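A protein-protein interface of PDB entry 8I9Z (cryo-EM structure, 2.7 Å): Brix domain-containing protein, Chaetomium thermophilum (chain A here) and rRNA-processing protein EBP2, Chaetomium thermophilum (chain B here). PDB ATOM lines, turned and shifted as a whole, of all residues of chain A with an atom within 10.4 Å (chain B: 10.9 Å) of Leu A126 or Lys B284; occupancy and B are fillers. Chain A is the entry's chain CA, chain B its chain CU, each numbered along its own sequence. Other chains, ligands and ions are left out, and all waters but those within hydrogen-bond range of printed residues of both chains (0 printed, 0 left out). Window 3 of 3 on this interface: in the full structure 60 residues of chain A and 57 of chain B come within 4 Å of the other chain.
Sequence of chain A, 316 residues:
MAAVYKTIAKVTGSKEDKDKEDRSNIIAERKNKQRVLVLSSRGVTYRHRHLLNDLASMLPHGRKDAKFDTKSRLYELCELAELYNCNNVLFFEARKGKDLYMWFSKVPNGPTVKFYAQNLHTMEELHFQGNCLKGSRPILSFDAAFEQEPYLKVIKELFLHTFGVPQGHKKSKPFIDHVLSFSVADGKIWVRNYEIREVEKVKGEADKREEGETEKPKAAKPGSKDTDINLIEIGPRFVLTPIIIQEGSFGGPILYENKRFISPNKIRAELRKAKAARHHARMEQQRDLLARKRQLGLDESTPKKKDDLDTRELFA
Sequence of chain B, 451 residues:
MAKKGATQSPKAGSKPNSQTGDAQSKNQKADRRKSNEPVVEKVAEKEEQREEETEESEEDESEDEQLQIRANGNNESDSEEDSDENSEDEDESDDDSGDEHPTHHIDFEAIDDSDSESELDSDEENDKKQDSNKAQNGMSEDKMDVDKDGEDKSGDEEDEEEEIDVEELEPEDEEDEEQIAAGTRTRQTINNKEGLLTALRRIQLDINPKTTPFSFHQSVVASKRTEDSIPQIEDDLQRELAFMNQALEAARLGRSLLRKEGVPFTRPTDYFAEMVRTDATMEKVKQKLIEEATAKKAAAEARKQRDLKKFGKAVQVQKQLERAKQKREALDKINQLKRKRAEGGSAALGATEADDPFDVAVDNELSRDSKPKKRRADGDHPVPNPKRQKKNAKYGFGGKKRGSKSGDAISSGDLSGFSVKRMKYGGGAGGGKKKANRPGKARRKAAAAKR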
ATOM      1  N   ARG A  47      14.369 -31.238 -11.084  1.00  0.00           N
ATOM      2  CA  ARG A  47      13.049 -31.238 -11.702  1.00  0.00           C
ATOM      3  C   ARG A  47      12.317 -32.544 -11.432  1.00  0.00           C
ATOM      4  O   ARG A  47      11.095 -32.551 -11.256  1.00  0.00           O
ATOM      5  CB  ARG A  47      13.175 -30.989 -13.204  1.00  0.00           C
ATOM      6  CG  ARG A  47      11.865 -30.664 -13.888  1.00  0.00           C
ATOM      7  CD  ARG A  47      12.089 -30.244 -15.327  1.00  0.00           C
ATOM      8  NE  ARG A  47      12.911 -29.044 -15.420  1.00  0.00           N
ATOM      9  CZ  ARG A  47      12.442 -27.807 -15.325  1.00  0.00           C
ATOM     10  NH1 ARG A  47      11.154 -27.568 -15.137  1.00  0.00           N
ATOM     11  NH2 ARG A  47      13.287 -26.785 -15.424  1.00  0.00           N
ATOM     12  N   HIS A 121       6.507 -30.124 -16.155  1.00  0.00           N
ATOM     13  CA  HIS A 121       6.252 -28.752 -15.728  1.00  0.00           C
ATOM     14  C   HIS A 121       5.631 -28.805 -14.341  1.00  0.00           C
ATOM     15  O   HIS A 121       4.494 -29.256 -14.187  1.00  0.00           O
ATOM     16  CB  HIS A 121       5.334 -28.025 -16.710  1.00  0.00           C
ATOM     17  CG  HIS A 121       5.995 -27.662 -18.001  1.00  0.00           C
ATOM     18  ND1 HIS A 121       6.755 -26.524 -18.152  1.00  0.00           N
ATOM     19  CD2 HIS A 121       6.002 -28.282 -19.204  1.00  0.00           C
ATOM     20  CE1 HIS A 121       7.207 -26.460 -19.391  1.00  0.00           C
ATOM     21  NE2 HIS A 121       6.765 -27.516 -20.049  1.00  0.00           N
ATOM     22  N   THR A 122       6.365 -28.337 -13.337  1.00  0.00           N
ATOM     23  CA  THR A 122       5.966 -28.497 -11.948  1.00  0.00           C
ATOM     24  C   THR A 122       5.120 -27.312 -11.473  1.00  0.00           C
ATOM     25  O   THR A 122       4.867 -26.358 -12.210  1.00  0.00           O
ATOM     26  CB  THR A 122       7.201 -28.682 -11.073  1.00  0.00           C
ATOM     27  OG1 THR A 122       7.954 -27.465 -11.037  1.00  0.00           O
ATOM     28  CG2 THR A 122       8.069 -29.792 -11.632  1.00  0.00           C
ATOM     29  N   MET A 123       4.684 -27.381 -10.208  1.00  0.00           N
ATOM     30  CA  MET A 123       3.768 -26.385  -9.653  1.00  0.00           C
ATOM     31  C   MET A 123       4.424 -25.024  -9.472  1.00  0.00           C
ATOM     32  O   MET A 123       3.738 -23.998  -9.530  1.00  0.00           O
ATOM     33  CB  MET A 123       3.220 -26.850  -8.305  1.00  0.00           C
ATOM     34  CG  MET A 123       1.922 -27.616  -8.378  1.00  0.00           C
ATOM     35  SD  MET A 123       1.763 -28.838  -7.073  1.00  0.00           S
ATOM     36  CE  MET A 123       0.161 -29.529  -7.462  1.00  0.00           C
ATOM     37  N   GLU A 124       5.735 -24.987  -9.252  1.00  0.00           N
ATOM     38  CA  GLU A 124       6.429 -23.736  -8.979  1.00  0.00           C
ATOM     39  C   GLU A 124       6.538 -22.826 -10.193  1.00  0.00           C
ATOM     40  O   GLU A 124       6.958 -21.676 -10.032  1.00  0.00           O
ATOM     41  CB  GLU A 124       7.829 -24.021  -8.422  1.00  0.00           C
ATOM     42  CG  GLU A 124       7.955 -24.382  -6.913  1.00  0.00           C
ATOM     43  CD  GLU A 124       7.020 -25.479  -6.366  1.00  0.00           C
ATOM     44  OE1 GLU A 124       6.361 -26.222  -7.127  1.00  0.00           O
ATOM     45  OE2 GLU A 124       6.947 -25.594  -5.125  1.00  0.00           O
ATOM     46  N   GLU A 125       6.186 -23.296 -11.386  1.00  0.00           N
ATOM     47  CA  GLU A 125       6.226 -22.450 -12.572  1.00  0.00           C
ATOM     48  C   GLU A 125       5.082 -21.445 -12.530  1.00  0.00           C
ATOM     49  O   GLU A 125       3.914 -21.825 -12.427  1.00  0.00           O
ATOM     50  CB  GLU A 125       6.152 -23.308 -13.829  1.00  0.00           C
ATOM     51  CG  GLU A 125       7.262 -24.339 -13.919  1.00  0.00           C
ATOM     52  CD  GLU A 125       7.478 -24.841 -15.330  1.00  0.00           C
ATOM     53  OE1 GLU A 125       7.050 -24.152 -16.280  1.00  0.00           O
ATOM     54  OE2 GLU A 125       8.082 -25.922 -15.490  1.00  0.00           O
ATOM     55  N   LEU A 126       5.421 -20.161 -12.625  1.00  0.00           N
ATOM     56  CA  LEU A 126       4.468 -19.075 -12.399  1.00  0.00           C
ATOM     57  C   LEU A 126       3.624 -18.746 -13.620  1.00  0.00           C
ATOM     58  O   LEU A 126       3.473 -17.575 -13.970  1.00  0.00           O
ATOM     59  CB  LEU A 126       5.228 -17.836 -11.932  1.00  0.00           C
ATOM     60  CG  LEU A 126       6.269 -18.011 -10.830  1.00  0.00           C
ATOM     61  CD1 LEU A 126       7.055 -16.729 -10.657  1.00  0.00           C
ATOM     62  CD2 LEU A 126       5.608 -18.412  -9.526  1.00  0.00           C
ATOM     63  N   HIS A 127       3.045 -19.746 -14.276  1.00  0.00           N
ATOM     64  CA  HIS A 127       2.172 -19.498 -15.416  1.00  0.00           C
ATOM     65  C   HIS A 127       0.907 -20.337 -15.336  1.00  0.00           C
ATOM     66  O   HIS A 127       0.197 -20.479 -16.337  1.00  0.00           O
ATOM     67  CB  HIS A 127       2.900 -19.764 -16.739  1.00  0.00           C
ATOM     68  CG  HIS A 127       3.141 -21.214 -17.018  1.00  0.00           C
ATOM     69  ND1 HIS A 127       2.628 -21.854 -18.125  1.00  0.00           N
ATOM     70  CD2 HIS A 127       3.842 -22.150 -16.336  1.00  0.00           C
ATOM     71  CE1 HIS A 127       3.001 -23.122 -18.112  1.00  0.00           C
ATOM     72  NE2 HIS A 127       3.739 -23.326 -17.038  1.00  0.00           N
ATOM     73  N   PHE A 128       0.606 -20.885 -14.163  1.00  0.00           N
ATOM     74  CA  PHE A 128      -0.495 -21.828 -14.036  1.00  0.00           C
ATOM     75  C   PHE A 128      -1.761 -21.181 -13.486  1.00  0.00           C
ATOM     76  O   PHE A 128      -2.860 -21.485 -13.959  1.00  0.00           O
ATOM     77  CB  PHE A 128      -0.057 -23.006 -13.170  1.00  0.00           C
ATOM     78  CG  PHE A 128       0.676 -24.067 -13.933  1.00  0.00           C
ATOM     79  CD1 PHE A 128       0.277 -24.407 -15.213  1.00  0.00           C
ATOM     80  CD2 PHE A 128       1.761 -24.716 -13.384  1.00  0.00           C
ATOM     81  CE1 PHE A 128       0.941 -25.376 -15.925  1.00  0.00           C
ATOM     82  CE2 PHE A 128       2.428 -25.688 -14.095  1.00  0.00           C
ATOM     83  CZ  PHE A 128       2.017 -26.016 -15.365  1.00  0.00           C
ATOM     84  N   GLN A 129      -1.619 -20.306 -12.488  1.00  0.00           N
ATOM     85  CA  GLN A 129      -2.674 -19.492 -11.880  1.00  0.00           C
ATOM     86  C   GLN A 129      -3.715 -20.313 -11.129  1.00  0.00           C
ATOM     87  O   GLN A 129      -4.749 -19.767 -10.734  1.00  0.00           O
ATOM     88  CB  GLN A 129      -3.402 -18.627 -12.915  1.00  0.00           C
ATOM     89  CG  GLN A 129      -2.506 -17.766 -13.756  1.00  0.00           C
ATOM     90  CD  GLN A 129      -3.272 -17.070 -14.850  1.00  0.00           C
ATOM     91  OE1 GLN A 129      -4.427 -17.393 -15.115  1.00  0.00           O
ATOM     92  NE2 GLN A 129      -2.612 -16.162 -15.543  1.00  0.00           N
ATOM     93  N   GLY A 130      -3.483 -21.601 -10.914  1.00  0.00           N
ATOM     94  CA  GLY A 130      -4.455 -22.460 -10.267  1.00  0.00           C
ATOM     95  C   GLY A 130      -3.895 -23.070  -9.000  1.00  0.00           C
ATOM     96  O   GLY A 130      -2.696 -23.318  -8.891  1.00  0.00           O
ATOM     97  N   ASN A 131      -4.779 -23.309  -8.036  1.00  0.00           N
ATOM     98  CA  ASN A 131      -4.410 -23.882  -6.753  1.00  0.00           C
ATOM     99  C   ASN A 131      -5.595 -24.658  -6.204  1.00  0.00           C
ATOM    100  O   ASN A 131      -6.748 -24.360  -6.521  1.00  0.00           O
ATOM    101  CB  ASN A 131      -3.974 -22.803  -5.762  1.00  0.00           C
ATOM    102  CG  ASN A 131      -3.041 -23.325  -4.700  1.00  0.00           C
ATOM    103  OD1 ASN A 131      -2.916 -24.528  -4.512  1.00  0.00           O
ATOM    104  ND2 ASN A 131      -2.384 -22.420  -3.992  1.00  0.00           N
ATOM    105  N   GLU A 233      -5.675 -24.529 -14.889  1.00  0.00           N
ATOM    106  CA  GLU A 233      -4.626 -25.521 -14.706  1.00  0.00           C
ATOM    107  C   GLU A 233      -3.829 -25.233 -13.440  1.00  0.00           C
ATOM    108  O   GLU A 233      -3.419 -24.098 -13.199  1.00  0.00           O
ATOM    109  CB  GLU A 233      -3.713 -25.511 -15.927  1.00  0.00           C
ATOM    110  CG  GLU A 233      -3.353 -26.871 -16.454  1.00  0.00           C
ATOM    111  CD  GLU A 233      -2.008 -26.887 -17.127  1.00  0.00           C
ATOM    112  OE1 GLU A 233      -1.715 -25.953 -17.902  1.00  0.00           O
ATOM    113  OE2 GLU A 233      -1.243 -27.839 -16.883  1.00  0.00           O
ATOM    114  N   ILE A 234      -3.605 -26.262 -12.627  1.00  0.00           N
ATOM    115  CA  ILE A 234      -2.920 -26.065 -11.353  1.00  0.00           C
ATOM    116  C   ILE A 234      -1.471 -26.498 -11.450  1.00  0.00           C
ATOM    117  O   ILE A 234      -0.553 -25.687 -11.299  1.00  0.00           O
ATOM    118  CB  ILE A 234      -3.596 -26.839 -10.208  1.00  0.00           C
ATOM    119  CG1 ILE A 234      -5.059 -26.458 -10.071  1.00  0.00           C
ATOM    120  CG2 ILE A 234      -2.851 -26.622  -8.906  1.00  0.00           C
ATOM    121  CD1 ILE A 234      -5.814 -27.398  -9.197  1.00  0.00           C
ATOM    122  N   GLY A 235      -1.260 -27.782 -11.697  1.00  0.00           N
ATOM    123  CA  GLY A 235      -0.024 -28.401 -11.313  1.00  0.00           C
ATOM    124  C   GLY A 235       0.706 -29.121 -12.413  1.00  0.00           C
ATOM    125  O   GLY A 235       0.931 -28.591 -13.505  1.00  0.00           O
ATOM    126  N   ARG B 277      -0.014 -25.370  -3.476  1.00  0.00           N
ATOM    127  CA  ARG B 277       0.933 -24.297  -3.733  1.00  0.00           C
ATOM    128  C   ARG B 277       0.814 -23.254  -2.636  1.00  0.00           C
ATOM    129  O   ARG B 277      -0.291 -22.857  -2.261  1.00  0.00           O
ATOM    130  CB  ARG B 277       0.679 -23.666  -5.097  1.00  0.00           C
ATOM    131  CG  ARG B 277       0.523 -24.683  -6.200  1.00  0.00           C
ATOM    132  CD  ARG B 277       0.101 -24.037  -7.492  1.00  0.00           C
ATOM    133  NE  ARG B 277       1.139 -23.190  -8.058  1.00  0.00           N
ATOM    134  CZ  ARG B 277       0.997 -22.486  -9.171  1.00  0.00           C
ATOM    135  NH1 ARG B 277      -0.136 -22.489  -9.849  1.00  0.00           N
ATOM    136  NH2 ARG B 277       2.017 -21.758  -9.611  1.00  0.00           N
ATOM    137  N   THR B 278       1.958 -22.817  -2.122  1.00  0.00           N
ATOM    138  CA  THR B 278       1.991 -21.948  -0.960  1.00  0.00           C
ATOM    139  C   THR B 278       1.498 -20.547  -1.316  1.00  0.00           C
ATOM    140  O   THR B 278       1.398 -20.169  -2.485  1.00  0.00           O
ATOM    141  CB  THR B 278       3.402 -21.886  -0.383  1.00  0.00           C
ATOM    142  OG1 THR B 278       4.278 -21.266  -1.330  1.00  0.00           O
ATOM    143  CG2 THR B 278       3.907 -23.281  -0.082  1.00  0.00           C
ATOM    144  N   ASP B 279       1.175 -19.777  -0.272  1.00  0.00           N
ATOM    145  CA  ASP B 279       0.764 -18.390  -0.466  1.00  0.00           C
ATOM    146  C   ASP B 279       1.915 -17.551  -0.998  1.00  0.00           C
ATOM    147  O   ASP B 279       1.696 -16.550  -1.688  1.00  0.00           O
ATOM    148  CB  ASP B 279       0.243 -17.806   0.844  1.00  0.00           C
ATOM    149  CG  ASP B 279      -1.135 -18.312   1.200  1.00  0.00           C
ATOM    150  OD1 ASP B 279      -1.554 -19.345   0.638  1.00  0.00           O
ATOM    151  OD2 ASP B 279      -1.800 -17.679   2.043  1.00  0.00           O
ATOM    152  N   ALA B 280       3.149 -17.934  -0.666  1.00  0.00           N
ATOM    153  CA  ALA B 280       4.312 -17.271  -1.241  1.00  0.00           C
ATOM    154  C   ALA B 280       4.379 -17.492  -2.746  1.00  0.00           C
ATOM    155  O   ALA B 280       4.706 -16.569  -3.498  1.00  0.00           O
ATOM    156  CB  ALA B 280       5.587 -17.767  -0.564  1.00  0.00           C
ATOM    157  N   THR B 281       4.069 -18.707  -3.205  1.00  0.00           N
ATOM    158  CA  THR B 281       4.067 -18.989  -4.639  1.00  0.00           C
ATOM    159  C   THR B 281       2.928 -18.264  -5.343  1.00  0.00           C
ATOM    160  O   THR B 281       3.112 -17.729  -6.443  1.00  0.00           O
ATOM    161  CB  THR B 281       3.976 -20.496  -4.876  1.00  0.00           C
ATOM    162  OG1 THR B 281       5.042 -21.148  -4.177  1.00  0.00           O
ATOM    163  CG2 THR B 281       4.079 -20.826  -6.356  1.00  0.00           C
ATOM    164  N   MET B 282       1.749 -18.228  -4.721  1.00  0.00           N
ATOM    165  CA  MET B 282       0.617 -17.481  -5.258  1.00  0.00           C
ATOM    166  C   MET B 282       0.880 -15.984  -5.319  1.00  0.00           C
ATOM    167  O   MET B 282       0.275 -15.292  -6.144  1.00  0.00           O
ATOM    168  CB  MET B 282      -0.633 -17.752  -4.419  1.00  0.00           C
ATOM    169  CG  MET B 282      -1.239 -19.167  -4.451  1.00  0.00           C
ATOM    170  SD  MET B 282      -1.963 -19.765  -6.004  1.00  0.00           S
ATOM    171  CE  MET B 282      -0.584 -20.327  -6.982  1.00  0.00           C
ATOM    172  N   GLU B 283       1.752 -15.468  -4.455  1.00  0.00           N
ATOM    173  CA  GLU B 283       2.097 -14.053  -4.519  1.00  0.00           C
ATOM    174  C   GLU B 283       2.912 -13.742  -5.765  1.00  0.00           C
ATOM    175  O   GLU B 283       2.694 -12.715  -6.415  1.00  0.00           O
ATOM    176  CB  GLU B 283       2.850 -13.642  -3.260  1.00  0.00           C
ATOM    177  CG  GLU B 283       2.103 -12.632  -2.412  1.00  0.00           C
ATOM    178  CD  GLU B 283       1.942 -11.292  -3.102  1.00  0.00           C
ATOM    179  OE1 GLU B 283       2.862 -10.884  -3.841  1.00  0.00           O
ATOM    180  OE2 GLU B 283       0.890 -10.647  -2.912  1.00  0.00           O
ATOM    181  N   LYS B 284       3.848 -14.622  -6.124  1.00  0.00           N
ATOM    182  CA  LYS B 284       4.646 -14.404  -7.326  1.00  0.00           C
ATOM    183  C   LYS B 284       3.812 -14.579  -8.588  1.00  0.00           C
ATOM    184  O   LYS B 284       4.112 -13.978  -9.626  1.00  0.00           O
ATOM    185  CB  LYS B 284       5.847 -15.347  -7.337  1.00  0.00           C
ATOM    186  CG  LYS B 284       6.449 -15.579  -5.977  1.00  0.00           C
ATOM    187  CD  LYS B 284       7.958 -15.560  -6.026  1.00  0.00           C
ATOM    188  CE  LYS B 284       8.506 -16.944  -6.314  1.00  0.00           C
ATOM    189  NZ  LYS B 284       8.468 -17.813  -5.110  1.00  0.00           N
ATOM    190  N   VAL B 285       2.772 -15.411  -8.524  1.00  0.00           N
ATOM    191  CA  VAL B 285       1.849 -15.547  -9.647  1.00  0.00           C
ATOM    192  C   VAL B 285       1.069 -14.254  -9.844  1.00  0.00           C
ATOM    193  O   VAL B 285       0.884 -13.783 -10.973  1.00  0.00           O
ATOM    194  CB  VAL B 285       0.914 -16.751  -9.425  1.00  0.00           C
ATOM    195  CG1 VAL B 285      -0.190 -16.783 -10.465  1.00  0.00           C
ATOM    196  CG2 VAL B 285       1.705 -18.042  -9.454  1.00  0.00           C
ATOM    197  N   LYS B 286       0.614 -13.652  -8.744  1.00  0.00           N
ATOM    198  CA  LYS B 286      -0.143 -12.408  -8.838  1.00  0.00           C
ATOM    199  C   LYS B 286       0.739 -11.245  -9.272  1.00  0.00           C
ATOM    200  O   LYS B 286       0.302 -10.388 -10.047  1.00  0.00           O
ATOM    201  CB  LYS B 286      -0.815 -12.095  -7.505  1.00  0.00           C
ATOM    202  CG  LYS B 286      -2.136 -11.365  -7.643  1.00  0.00           C
ATOM    203  CD  LYS B 286      -2.679 -10.953  -6.290  1.00  0.00           C
ATOM    204  CE  LYS B 286      -2.448  -9.476  -6.026  1.00  0.00           C
ATOM    205  NZ  LYS B 286      -2.853  -8.633  -7.185  1.00  0.00           N
ATOM    206  N   GLN B 287       1.978 -11.188  -8.780  1.00  0.00           N
ATOM    207  CA  GLN B 287       2.870 -10.102  -9.172  1.00  0.00           C
ATOM    208  C   GLN B 287       3.297 -10.232 -10.626  1.00  0.00           C
ATOM    209  O   GLN B 287       3.560  -9.224 -11.291  1.00  0.00           O
ATOM    210  CB  GLN B 287       4.093 -10.057  -8.258  1.00  0.00           C
ATOM    211  CG  GLN B 287       3.790  -9.728  -6.806  1.00  0.00           C
ATOM    212  CD  GLN B 287       3.106  -8.383  -6.615  1.00  0.00           C
ATOM    213  OE1 GLN B 287       3.309  -7.447  -7.390  1.00  0.00           O
ATOM    214  NE2 GLN B 287       2.289  -8.283  -5.574  1.00  0.00           N
ATOM    215  N   LYS B 288       3.387 -11.461 -11.134  1.00  0.00           N
ATOM    216  CA  LYS B 288       3.671 -11.645 -12.550  1.00  0.00           C
ATOM    217  C   LYS B 288       2.510 -11.164 -13.407  1.00  0.00           C
ATOM    218  O   LYS B 288       2.719 -10.565 -14.465  1.00  0.00           O
ATOM    219  CB  LYS B 288       3.988 -13.109 -12.843  1.00  0.00           C
ATOM    220  CG  LYS B 288       4.686 -13.324 -14.166  1.00  0.00           C
ATOM    221  CD  LYS B 288       5.101 -14.767 -14.346  1.00  0.00           C
ATOM    222  CE  LYS B 288       5.206 -15.139 -15.815  1.00  0.00           C
ATOM    223  NZ  LYS B 288       4.945 -13.987 -16.719  1.00  0.00           N
ATOM    224  N   LEU B 289       1.276 -11.409 -12.960  1.00  0.00           N
ATOM    225  CA  LEU B 289       0.107 -10.970 -13.716  1.00  0.00           C
ATOM    226  C   LEU B 289      -0.020  -9.455 -13.723  1.00  0.00           C
ATOM    227  O   LEU B 289      -0.516  -8.874 -14.693  1.00  0.00           O
ATOM    228  CB  LEU B 289      -1.158 -11.599 -13.146  1.00  0.00           C
ATOM    229  CG  LEU B 289      -1.365 -13.050 -13.540  1.00  0.00           C
ATOM    230  CD1 LEU B 289      -2.478 -13.671 -12.726  1.00  0.00           C
ATOM    231  CD2 LEU B 289      -1.684 -13.065 -15.012  1.00  0.00           C
ATOM    232  N   ILE B 290       0.396  -8.803 -12.639  1.00  0.00           N
ATOM    233  CA  ILE B 290       0.378  -7.345 -12.595  1.00  0.00           C
ATOM    234  C   ILE B 290       1.383  -6.778 -13.590  1.00  0.00           C
ATOM    235  O   ILE B 290       1.120  -5.771 -14.259  1.00  0.00           O
ATOM    236  CB  ILE B 290       0.648  -6.865 -11.155  1.00  0.00           C
ATOM    237  CG1 ILE B 290      -0.533  -7.214 -10.250  1.00  0.00           C
ATOM    238  CG2 ILE B 290       0.931  -5.368 -11.101  1.00  0.00           C
ATOM    239  CD1 ILE B 290      -1.764  -6.378 -10.485  1.00  0.00           C
ATOM    240  N   GLU B 291       2.531  -7.444 -13.732  1.00  0.00           N
ATOM    241  CA  GLU B 291       3.601  -6.939 -14.585  1.00  0.00           C
ATOM    242  C   GLU B 291       3.205  -6.947 -16.059  1.00  0.00           C
ATOM    243  O   GLU B 291       3.461  -5.977 -16.781  1.00  0.00           O
ATOM    244  CB  GLU B 291       4.874  -7.755 -14.362  1.00  0.00           C
ATOM    245  CG  GLU B 291       5.620  -7.392 -13.091  1.00  0.00           C
ATOM    246  CD  GLU B 291       7.093  -7.744 -13.161  1.00  0.00           C
ATOM    247  OE1 GLU B 291       7.456  -8.633 -13.959  1.00  0.00           O
ATOM    248  OE2 GLU B 291       7.888  -7.132 -12.416  1.00  0.00           O
ATOM    249  N   GLU B 292       2.585  -8.031 -16.529  1.00  0.00           N
ATOM    250  CA  GLU B 292       2.145  -8.064 -17.921  1.00  0.00           C
ATOM    251  C   GLU B 292       0.946  -7.155 -18.148  1.00  0.00           C
ATOM    252  O   GLU B 292       0.790  -6.586 -19.233  1.00  0.00           O
ATOM    253  CB  GLU B 292       1.817  -9.491 -18.356  1.00  0.00           C
ATOM    254  CG  GLU B 292       2.607 -10.573 -17.664  1.00  0.00           C
ATOM    255  CD  GLU B 292       2.946 -11.722 -18.593  1.00  0.00           C
ATOM    256  OE1 GLU B 292       2.300 -11.840 -19.655  1.00  0.00           O
ATOM    257  OE2 GLU B 292       3.856 -12.508 -18.260  1.00  0.00           O
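The backbone carbonyl oxygen of Met A123 is in hydrogen-bond range of the guanidinium group of Arg B277, at 2.8 Å. The guanidinium group (NH2) of Arg B277 is in hydrogen-bond range of the backbone carbonyl oxygen (O) of Glu A125 (3.4 Å). The backbone carbonyl oxygen (O) of Gly A130 lies within hydrogen-bond range of the guanidinium group (NH1) of Arg B277, at 2.9 Å. The backbone carbonyl oxygen of Arg B277 sits at hydrogen-bond distance from the side-chain amide nitrogen of Asn A131 (2.8 Å). SD of Met B282 is in hydrogen-bond range of ND2 of Asn A131.
The side-chain carboxylate of Glu A125 lies within salt-bridge range of the guanidinium group of Arg A47, 3.5 Å away. ND1 of His A121 lies within hydrogen-bond range of OE2 of Glu A125, 3.0 Å away. OE1 of Glu A125 is in hydrogen-bond range of NE2 of His A127 (3.5 Å). O of Glu A233 lies within hydrogen-bond range of N of Gly A130 (3.4 Å).
Among the printed residues, pairs that only touch across the chains: Leu A126 with Lys B288 (3.3 Å), Gln A129 with Leu B289 (3.3 Å), Phe A128 with Arg B277 (3.4 Å), Ile A234 with Arg B277 (3.5 Å), Gln A129 with Arg B277 (3.7 Å), Leu A126 with Lys B284 (3.8 Å), Leu A126 with Val B285 (3.9 Å) and Gln A129 with Val B285 (3.9 Å).
Leu A126 touches just these residues of chain B: Lys B284 (3.8 Å), Val B285 (3.9 Å) and Lys B288 (3.3 Å). Lys B284 touches just one residue of chain A: Leu A126 (3.8 Å). No residue of chain A comes within 4 Å of Glu B283. Lys B288 touches just one residue of chain A: Leu A126. Of the printed residues of chain A, Leu B289 touches Gln A129 (3.3 Å). Of the printed residues of chain B, Met A123 touches Arg B277 (2.8 Å). Printed residues of chain B within 4 Å of Asn A131: Arg B277 (2.8 Å) and Met B282 (3.4 Å). Printed residues of chain A within 4 Å of Met B282: Asn A131. Glu A124 touches none of the printed residues of chain B. The nearest residue of chain B that does not touch Leu A126 is Thr B281 (4.03 Å). The nearest printed residue of chain B that does not touch Asn A131 is Thr B278 (4.7 Å).
Printed residues of chain A that touch a printed residue of chain B: Met A123, Glu A125, Leu A126, Phe A128, Gln A129, Gly A130, Asn A131 and Ile A234. Of the 16 printed residues of chain B, 6 touch a printed residue of chain A. Printed residues of chain B that touch a printed residue of chain A: Arg B277, Met B282, Lys B284, Val B285, Lys B288 and Leu B289. Hydrophobic or aromatic side chains of chain B that line the printed part of chain A: Met B282, Val B285 and Leu B289.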
